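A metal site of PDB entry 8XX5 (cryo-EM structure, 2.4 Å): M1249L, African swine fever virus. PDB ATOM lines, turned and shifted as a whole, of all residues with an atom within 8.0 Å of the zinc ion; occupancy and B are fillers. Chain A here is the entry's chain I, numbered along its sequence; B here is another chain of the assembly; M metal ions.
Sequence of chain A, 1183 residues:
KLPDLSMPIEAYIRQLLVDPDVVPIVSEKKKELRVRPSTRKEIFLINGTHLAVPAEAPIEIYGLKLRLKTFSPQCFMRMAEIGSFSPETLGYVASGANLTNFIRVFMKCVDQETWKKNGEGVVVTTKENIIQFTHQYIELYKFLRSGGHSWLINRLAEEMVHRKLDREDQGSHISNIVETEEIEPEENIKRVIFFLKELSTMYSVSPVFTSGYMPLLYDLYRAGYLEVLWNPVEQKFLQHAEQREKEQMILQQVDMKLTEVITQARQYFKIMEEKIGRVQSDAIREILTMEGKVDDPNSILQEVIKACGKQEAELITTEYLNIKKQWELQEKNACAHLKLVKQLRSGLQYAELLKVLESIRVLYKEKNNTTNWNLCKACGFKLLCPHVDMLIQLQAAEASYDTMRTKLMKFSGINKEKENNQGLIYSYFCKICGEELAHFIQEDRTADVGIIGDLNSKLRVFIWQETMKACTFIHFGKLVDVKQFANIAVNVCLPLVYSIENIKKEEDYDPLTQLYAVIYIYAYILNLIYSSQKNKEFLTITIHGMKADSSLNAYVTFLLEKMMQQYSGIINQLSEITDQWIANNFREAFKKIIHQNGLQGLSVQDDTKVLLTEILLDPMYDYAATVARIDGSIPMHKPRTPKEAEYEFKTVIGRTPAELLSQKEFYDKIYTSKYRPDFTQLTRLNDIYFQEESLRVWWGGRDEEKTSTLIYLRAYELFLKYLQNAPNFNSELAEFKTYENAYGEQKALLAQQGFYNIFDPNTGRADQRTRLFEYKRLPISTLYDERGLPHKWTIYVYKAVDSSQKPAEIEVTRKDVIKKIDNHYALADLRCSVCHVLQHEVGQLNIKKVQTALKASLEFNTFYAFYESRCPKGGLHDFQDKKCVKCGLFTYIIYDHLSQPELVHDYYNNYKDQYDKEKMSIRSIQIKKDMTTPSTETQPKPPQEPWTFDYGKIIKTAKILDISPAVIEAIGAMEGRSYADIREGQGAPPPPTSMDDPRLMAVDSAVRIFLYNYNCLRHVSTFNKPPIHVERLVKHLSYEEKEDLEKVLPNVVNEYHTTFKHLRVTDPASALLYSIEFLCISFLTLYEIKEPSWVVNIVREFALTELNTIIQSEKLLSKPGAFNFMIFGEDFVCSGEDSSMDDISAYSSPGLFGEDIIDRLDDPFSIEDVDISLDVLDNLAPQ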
ATOM      1  N   ARG A 345      -7.733  27.155 -25.265  1.00  0.00           N
ATOM      2  CA  ARG A 345      -7.463  25.738 -25.108  1.00  0.00           C
ATOM      3  C   ARG A 345      -8.714  24.914 -24.863  1.00  0.00           C
ATOM      4  O   ARG A 345      -8.755  23.745 -25.274  1.00  0.00           O
ATOM      5  CB  ARG A 345      -6.464  25.516 -23.963  1.00  0.00           C
ATOM      6  CG  ARG A 345      -5.214  26.364 -24.074  1.00  0.00           C
ATOM      7  CD  ARG A 345      -4.491  26.073 -25.376  1.00  0.00           C
ATOM      8  NE  ARG A 345      -3.267  25.312 -25.161  1.00  0.00           N
ATOM      9  CZ  ARG A 345      -2.871  24.302 -25.924  1.00  0.00           C
ATOM     10  NH1 ARG A 345      -3.577  23.911 -26.979  1.00  0.00           N
ATOM     11  NH2 ARG A 345      -1.734  23.666 -25.632  1.00  0.00           N
ATOM     12  N   ASN A 372      11.237  31.784 -26.970  1.00  0.00           N
ATOM     13  CA  ASN A 372      10.869  31.745 -25.551  1.00  0.00           C
ATOM     14  C   ASN A 372       9.393  32.100 -25.447  1.00  0.00           C
ATOM     15  O   ASN A 372       8.688  32.244 -26.456  1.00  0.00           O
ATOM     16  CB  ASN A 372      11.741  32.696 -24.724  1.00  0.00           C
ATOM     17  CG  ASN A 372      13.028  32.055 -24.261  1.00  0.00           C
ATOM     18  OD1 ASN A 372      14.111  32.605 -24.428  1.00  0.00           O
ATOM     19  ND2 ASN A 372      12.924  30.862 -23.675  1.00  0.00           N
ATOM     20  N   TRP A 373       8.923  32.269 -24.206  1.00  0.00           N
ATOM     21  CA  TRP A 373       7.506  32.513 -23.939  1.00  0.00           C
ATOM     22  C   TRP A 373       7.067  33.865 -24.494  1.00  0.00           C
ATOM     23  O   TRP A 373       7.849  34.643 -25.045  1.00  0.00           O
ATOM     24  CB  TRP A 373       7.249  32.455 -22.434  1.00  0.00           C
ATOM     25  CG  TRP A 373       6.837  31.114 -21.913  1.00  0.00           C
ATOM     26  CD1 TRP A 373       7.666  30.113 -21.500  1.00  0.00           C
ATOM     27  CD2 TRP A 373       5.502  30.638 -21.713  1.00  0.00           C
ATOM     28  NE1 TRP A 373       6.926  29.037 -21.074  1.00  0.00           N
ATOM     29  CE2 TRP A 373       5.594  29.342 -21.196  1.00  0.00           C
ATOM     30  CE3 TRP A 373       4.237  31.185 -21.942  1.00  0.00           C
ATOM     31  CZ2 TRP A 373       4.478  28.574 -20.887  1.00  0.00           C
ATOM     32  CZ3 TRP A 373       3.126  30.430 -21.632  1.00  0.00           C
ATOM     33  CH2 TRP A 373       3.251  29.134 -21.116  1.00  0.00           C
ATOM     34  N   LEU A 384       1.485  33.033 -23.656  1.00  0.00           N
ATOM     35  CA  LEU A 384       1.253  31.917 -24.564  1.00  0.00           C
ATOM     36  C   LEU A 384       2.552  31.454 -25.219  1.00  0.00           C
ATOM     37  O   LEU A 384       3.336  32.285 -25.693  1.00  0.00           O
ATOM     38  CB  LEU A 384       0.230  32.306 -25.639  1.00  0.00           C
ATOM     39  CG  LEU A 384      -0.556  31.161 -26.267  1.00  0.00           C
ATOM     40  CD1 LEU A 384      -1.807  30.882 -25.444  1.00  0.00           C
ATOM     41  CD2 LEU A 384      -0.916  31.482 -27.706  1.00  0.00           C
ATOM     42  N   CYS A 385       2.776  30.150 -25.246  1.00  0.00           N
ATOM     43  CA  CYS A 385       3.977  29.615 -25.880  1.00  0.00           C
ATOM     44  C   CYS A 385       3.877  29.756 -27.402  1.00  0.00           C
ATOM     45  O   CYS A 385       2.786  29.688 -27.973  1.00  0.00           O
ATOM     46  CB  CYS A 385       4.159  28.153 -25.490  1.00  0.00           C
ATOM     47  SG  CYS A 385       5.323  27.238 -26.511  1.00  0.00           S
ATOM     48  N   PRO A 386       5.011  29.972 -28.076  1.00  0.00           N
ATOM     49  CA  PRO A 386       4.978  30.045 -29.547  1.00  0.00           C
ATOM     50  C   PRO A 386       4.430  28.793 -30.215  1.00  0.00           C
ATOM     51  O   PRO A 386       3.852  28.903 -31.301  1.00  0.00           O
ATOM     52  CB  PRO A 386       6.454  30.271 -29.915  1.00  0.00           C
ATOM     53  CG  PRO A 386       7.030  30.937 -28.721  1.00  0.00           C
ATOM     54  CD  PRO A 386       6.312  30.388 -27.527  1.00  0.00           C
ATOM     55  N   HIS A 387       4.616  27.610 -29.628  1.00  0.00           N
ATOM     56  CA  HIS A 387       4.106  26.395 -30.261  1.00  0.00           C
ATOM     57  C   HIS A 387       2.586  26.405 -30.290  1.00  0.00           C
ATOM     58  O   HIS A 387       1.980  25.823 -31.210  1.00  0.00           O
ATOM     59  CB  HIS A 387       4.615  25.152 -29.523  1.00  0.00           C
ATOM     60  CG  HIS A 387       3.663  24.591 -28.507  1.00  0.00           C
ATOM     61  ND1 HIS A 387       3.902  24.658 -27.148  1.00  0.00           N
ATOM     62  CD2 HIS A 387       2.515  23.890 -28.644  1.00  0.00           C
ATOM     63  CE1 HIS A 387       2.913  24.081 -26.500  1.00  0.00           C
ATOM     64  NE2 HIS A 387       2.057  23.604 -27.386  1.00  0.00           N
ATOM     65  N   VAL A 388       1.946  27.046 -29.314  1.00  0.00           N
ATOM     66  CA  VAL A 388       0.482  27.085 -29.280  1.00  0.00           C
ATOM     67  C   VAL A 388      -0.059  27.884 -30.461  1.00  0.00           C
ATOM     68  O   VAL A 388      -1.106  27.547 -31.030  1.00  0.00           O
ATOM     69  CB  VAL A 388      -0.008  27.651 -27.942  1.00  0.00           C
ATOM     70  CG1 VAL A 388      -1.514  27.500 -27.815  1.00  0.00           C
ATOM     71  CG2 VAL A 388       0.689  26.953 -26.789  1.00  0.00           C
ATOM     72  N   ASP A 389       0.652  28.943 -30.859  1.00  0.00           N
ATOM     73  CA  ASP A 389       0.250  29.710 -32.025  1.00  0.00           C
ATOM     74  C   ASP A 389       0.287  28.845 -33.286  1.00  0.00           C
ATOM     75  O   ASP A 389      -0.674  28.794 -34.054  1.00  0.00           O
ATOM     76  CB  ASP A 389       1.144  30.936 -32.182  1.00  0.00           C
ATOM     77  CG  ASP A 389       0.471  32.059 -32.955  1.00  0.00           C
ATOM     78  OD1 ASP A 389      -0.197  31.775 -33.968  1.00  0.00           O
ATOM     79  OD2 ASP A 389       0.624  33.232 -32.551  1.00  0.00           O
ATOM     80  N   LEU A 408       5.605  20.862 -35.937  1.00  0.00           N
ATOM     81  CA  LEU A 408       5.952  21.121 -34.543  1.00  0.00           C
ATOM     82  C   LEU A 408       7.326  20.573 -34.172  1.00  0.00           C
ATOM     83  O   LEU A 408       7.733  20.742 -33.018  1.00  0.00           O
ATOM     84  CB  LEU A 408       4.893  20.539 -33.605  1.00  0.00           C
ATOM     85  CG  LEU A 408       3.565  21.293 -33.532  1.00  0.00           C
ATOM     86  CD1 LEU A 408       2.511  20.451 -32.840  1.00  0.00           C
ATOM     87  CD2 LEU A 408       3.734  22.630 -32.831  1.00  0.00           C
ATOM     88  N   PHE A 411      10.042  22.892 -31.851  1.00  0.00           N
ATOM     89  CA  PHE A 411      10.016  23.125 -30.424  1.00  0.00           C
ATOM     90  C   PHE A 411      10.416  21.885 -29.630  1.00  0.00           C
ATOM     91  O   PHE A 411      10.211  21.841 -28.415  1.00  0.00           O
ATOM     92  CB  PHE A 411       8.636  23.601 -29.988  1.00  0.00           C
ATOM     93  CG  PHE A 411       8.061  24.695 -30.846  1.00  0.00           C
ATOM     94  CD1 PHE A 411       7.424  24.405 -32.036  1.00  0.00           C
ATOM     95  CD2 PHE A 411       8.148  26.015 -30.449  1.00  0.00           C
ATOM     96  CE1 PHE A 411       6.883  25.407 -32.822  1.00  0.00           C
ATOM     97  CE2 PHE A 411       7.613  27.029 -31.221  1.00  0.00           C
ATOM     98  CZ  PHE A 411       6.989  26.718 -32.411  1.00  0.00           C
ATOM     99  N   PHE A 429       8.205  16.693 -26.538  1.00  0.00           N
ATOM    100  CA  PHE A 429       7.796  17.725 -25.591  1.00  0.00           C
ATOM    101  C   PHE A 429       8.460  19.046 -25.955  1.00  0.00           C
ATOM    102  O   PHE A 429       9.563  19.075 -26.501  1.00  0.00           O
ATOM    103  CB  PHE A 429       8.139  17.319 -24.152  1.00  0.00           C
ATOM    104  CG  PHE A 429       7.321  16.169 -23.655  1.00  0.00           C
ATOM    105  CD1 PHE A 429       5.992  16.343 -23.302  1.00  0.00           C
ATOM    106  CD2 PHE A 429       7.879  14.902 -23.553  1.00  0.00           C
ATOM    107  CE1 PHE A 429       5.236  15.281 -22.841  1.00  0.00           C
ATOM    108  CE2 PHE A 429       7.122  13.840 -23.092  1.00  0.00           C
ATOM    109  CZ  PHE A 429       5.812  14.029 -22.732  1.00  0.00           C
ATOM    110  N   CYS A 430       7.765  20.136 -25.640  1.00  0.00           N
ATOM    111  CA  CYS A 430       8.197  21.453 -26.076  1.00  0.00           C
ATOM    112  C   CYS A 430       9.523  21.850 -25.434  1.00  0.00           C
ATOM    113  O   CYS A 430       9.774  21.577 -24.265  1.00  0.00           O
ATOM    114  CB  CYS A 430       7.131  22.500 -25.755  1.00  0.00           C
ATOM    115  SG  CYS A 430       7.514  24.117 -26.433  1.00  0.00           S
ATOM    116  N   LYS A 431      10.363  22.508 -26.239  1.00  0.00           N
ATOM    117  CA  LYS A 431      11.630  23.016 -25.719  1.00  0.00           C
ATOM    118  C   LYS A 431      11.418  24.239 -24.829  1.00  0.00           C
ATOM    119  O   LYS A 431      12.285  24.572 -24.013  1.00  0.00           O
ATOM    120  CB  LYS A 431      12.556  23.371 -26.890  1.00  0.00           C
ATOM    121  CG  LYS A 431      14.003  23.619 -26.516  1.00  0.00           C
ATOM    122  CD  LYS A 431      14.939  23.241 -27.654  1.00  0.00           C
ATOM    123  CE  LYS A 431      14.393  23.638 -29.017  1.00  0.00           C
ATOM    124  NZ  LYS A 431      14.122  25.102 -29.132  1.00  0.00           N
ATOM    125  N   ILE A 432      10.270  24.904 -24.959  1.00  0.00           N
ATOM    126  CA  ILE A 432       9.992  26.125 -24.224  1.00  0.00           C
ATOM    127  C   ILE A 432       9.186  25.794 -22.968  1.00  0.00           C
ATOM    128  O   ILE A 432       9.650  26.038 -21.850  1.00  0.00           O
ATOM    129  CB  ILE A 432       9.256  27.152 -25.096  1.00  0.00           C
ATOM    130  CG1 ILE A 432      10.187  27.715 -26.162  1.00  0.00           C
ATOM    131  CG2 ILE A 432       8.677  28.269 -24.243  1.00  0.00           C
ATOM    132  CD1 ILE A 432       9.842  27.292 -27.562  1.00  0.00           C
ATOM    133  N   CYS A 433       7.990  25.254 -23.148  1.00  0.00           N
ATOM    134  CA  CYS A 433       7.078  25.002 -22.035  1.00  0.00           C
ATOM    135  C   CYS A 433       6.968  23.524 -21.667  1.00  0.00           C
ATOM    136  O   CYS A 433       6.230  23.193 -20.736  1.00  0.00           O
ATOM    137  CB  CYS A 433       5.686  25.558 -22.363  1.00  0.00           C
ATOM    138  SG  CYS A 433       4.818  24.681 -23.672  1.00  0.00           S
ATOM    139  N   GLY A 434       7.660  22.636 -22.380  1.00  0.00           N
ATOM    140  CA  GLY A 434       7.615  21.230 -22.047  1.00  0.00           C
ATOM    141  C   GLY A 434       6.252  20.588 -22.206  1.00  0.00           C
ATOM    142  O   GLY A 434       5.889  19.722 -21.405  1.00  0.00           O
ATOM    143  N   GLU A 435       5.490  20.998 -23.210  1.00  0.00           N
ATOM    144  CA  GLU A 435       4.174  20.458 -23.469  1.00  0.00           C
ATOM    145  C   GLU A 435       4.243  19.377 -24.530  1.00  0.00           C
ATOM    146  O   GLU A 435       5.098  19.408 -25.417  1.00  0.00           O
ATOM    147  CB  GLU A 435       3.208  21.567 -23.911  1.00  0.00           C
ATOM    148  CG  GLU A 435       1.775  21.111 -24.058  1.00  0.00           C
ATOM    149  CD  GLU A 435       0.876  22.198 -24.620  1.00  0.00           C
ATOM    150  OE1 GLU A 435       0.470  23.088 -23.842  1.00  0.00           O
ATOM    151  OE2 GLU A 435       0.566  22.147 -25.823  1.00  0.00           O
ATOM    152  N   GLU A 436       3.334  18.406 -24.431  1.00  0.00           N
ATOM    153  CA  GLU A 436       3.251  17.355 -25.430  1.00  0.00           C
ATOM    154  C   GLU A 436       2.892  17.947 -26.793  1.00  0.00           C
ATOM    155  O   GLU A 436       1.790  18.467 -26.992  1.00  0.00           O
ATOM    156  CB  GLU A 436       2.248  16.280 -25.012  1.00  0.00           C
ATOM    157  CG  GLU A 436       0.836  16.778 -24.711  1.00  0.00           C
ATOM    158  CD  GLU A 436      -0.168  15.649 -24.583  1.00  0.00           C
ATOM    159  OE1 GLU A 436       0.104  14.540 -25.092  1.00  0.00           O
ATOM    160  OE2 GLU A 436      -1.236  15.868 -23.982  1.00  0.00           O
ATOM    161  N   LEU A 437       3.833  17.900 -27.728  1.00  0.00           N
ATOM    162  CA  LEU A 437       3.537  18.340 -29.089  1.00  0.00           C
ATOM    163  C   LEU A 437       2.763  17.267 -29.844  1.00  0.00           C
ATOM    164  O   LEU A 437       1.631  17.497 -30.290  1.00  0.00           O
ATOM    165  CB  LEU A 437       4.832  18.693 -29.827  1.00  0.00           C
ATOM    166  CG  LEU A 437       5.761  19.695 -29.141  1.00  0.00           C
ATOM    167  CD1 LEU A 437       7.190  19.523 -29.621  1.00  0.00           C
ATOM    168  CD2 LEU A 437       5.274  21.116 -29.385  1.00  0.00           C
ATOM    169  N   HIS B 388       2.118  17.859 -19.718  1.00  0.00           N
ATOM    170  CA  HIS B 388       3.406  18.527 -19.750  1.00  0.00           C
ATOM    171  C   HIS B 388       4.480  17.610 -19.173  1.00  0.00           C
ATOM    172  O   HIS B 388       4.263  16.951 -18.153  1.00  0.00           O
ATOM    173  CB  HIS B 388       3.365  19.836 -18.951  1.00  0.00           C
ATOM    174  CG  HIS B 388       2.653  20.946 -19.668  1.00  0.00           C
ATOM    175  ND1 HIS B 388       3.322  21.930 -20.363  1.00  0.00           N
ATOM    176  CD2 HIS B 388       1.337  21.236 -19.783  1.00  0.00           C
ATOM    177  CE1 HIS B 388       2.447  22.780 -20.874  1.00  0.00           C
ATOM    178  NE2 HIS B 388       1.228  22.369 -20.539  1.00  0.00           N
HETATM  179 ZN    ZN M   1       5.460  25.022 -25.876  1.00  0.00          ZN
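Along chain A the residues within 4 Å of the zinc ion span positions 385 to 433.
O of Cys 433 is in hydrogen-bond range of ND1 of His 388 of chain B (3.2 Å). NE2 of His 387 lies within hydrogen-bond range of OE2 of Glu 435 (2.6 Å). The side-chain sulfur of Cys 430 lies close to the backbone NH of Ile 432 (3.2 Å). N of Glu 435 lies close to SG of Cys 433 (3.8 Å). The backbone NH (N) of Cys 430 lies within hydrogen-bond range of the backbone carbonyl oxygen (O) of Glu 435, at 2.8 Å.
ND1 of His 387 binds the zinc ion. SG of Cys 385 is bound to the zinc ion, at 2.3 Å. The zinc ion is bound by SG of Cys 430, at 2.3 Å. The side-chain sulfur (SG) of Cys 433 binds the zinc ion, 2.3 Å away. The zinc ion has four donor atoms within binding distance.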
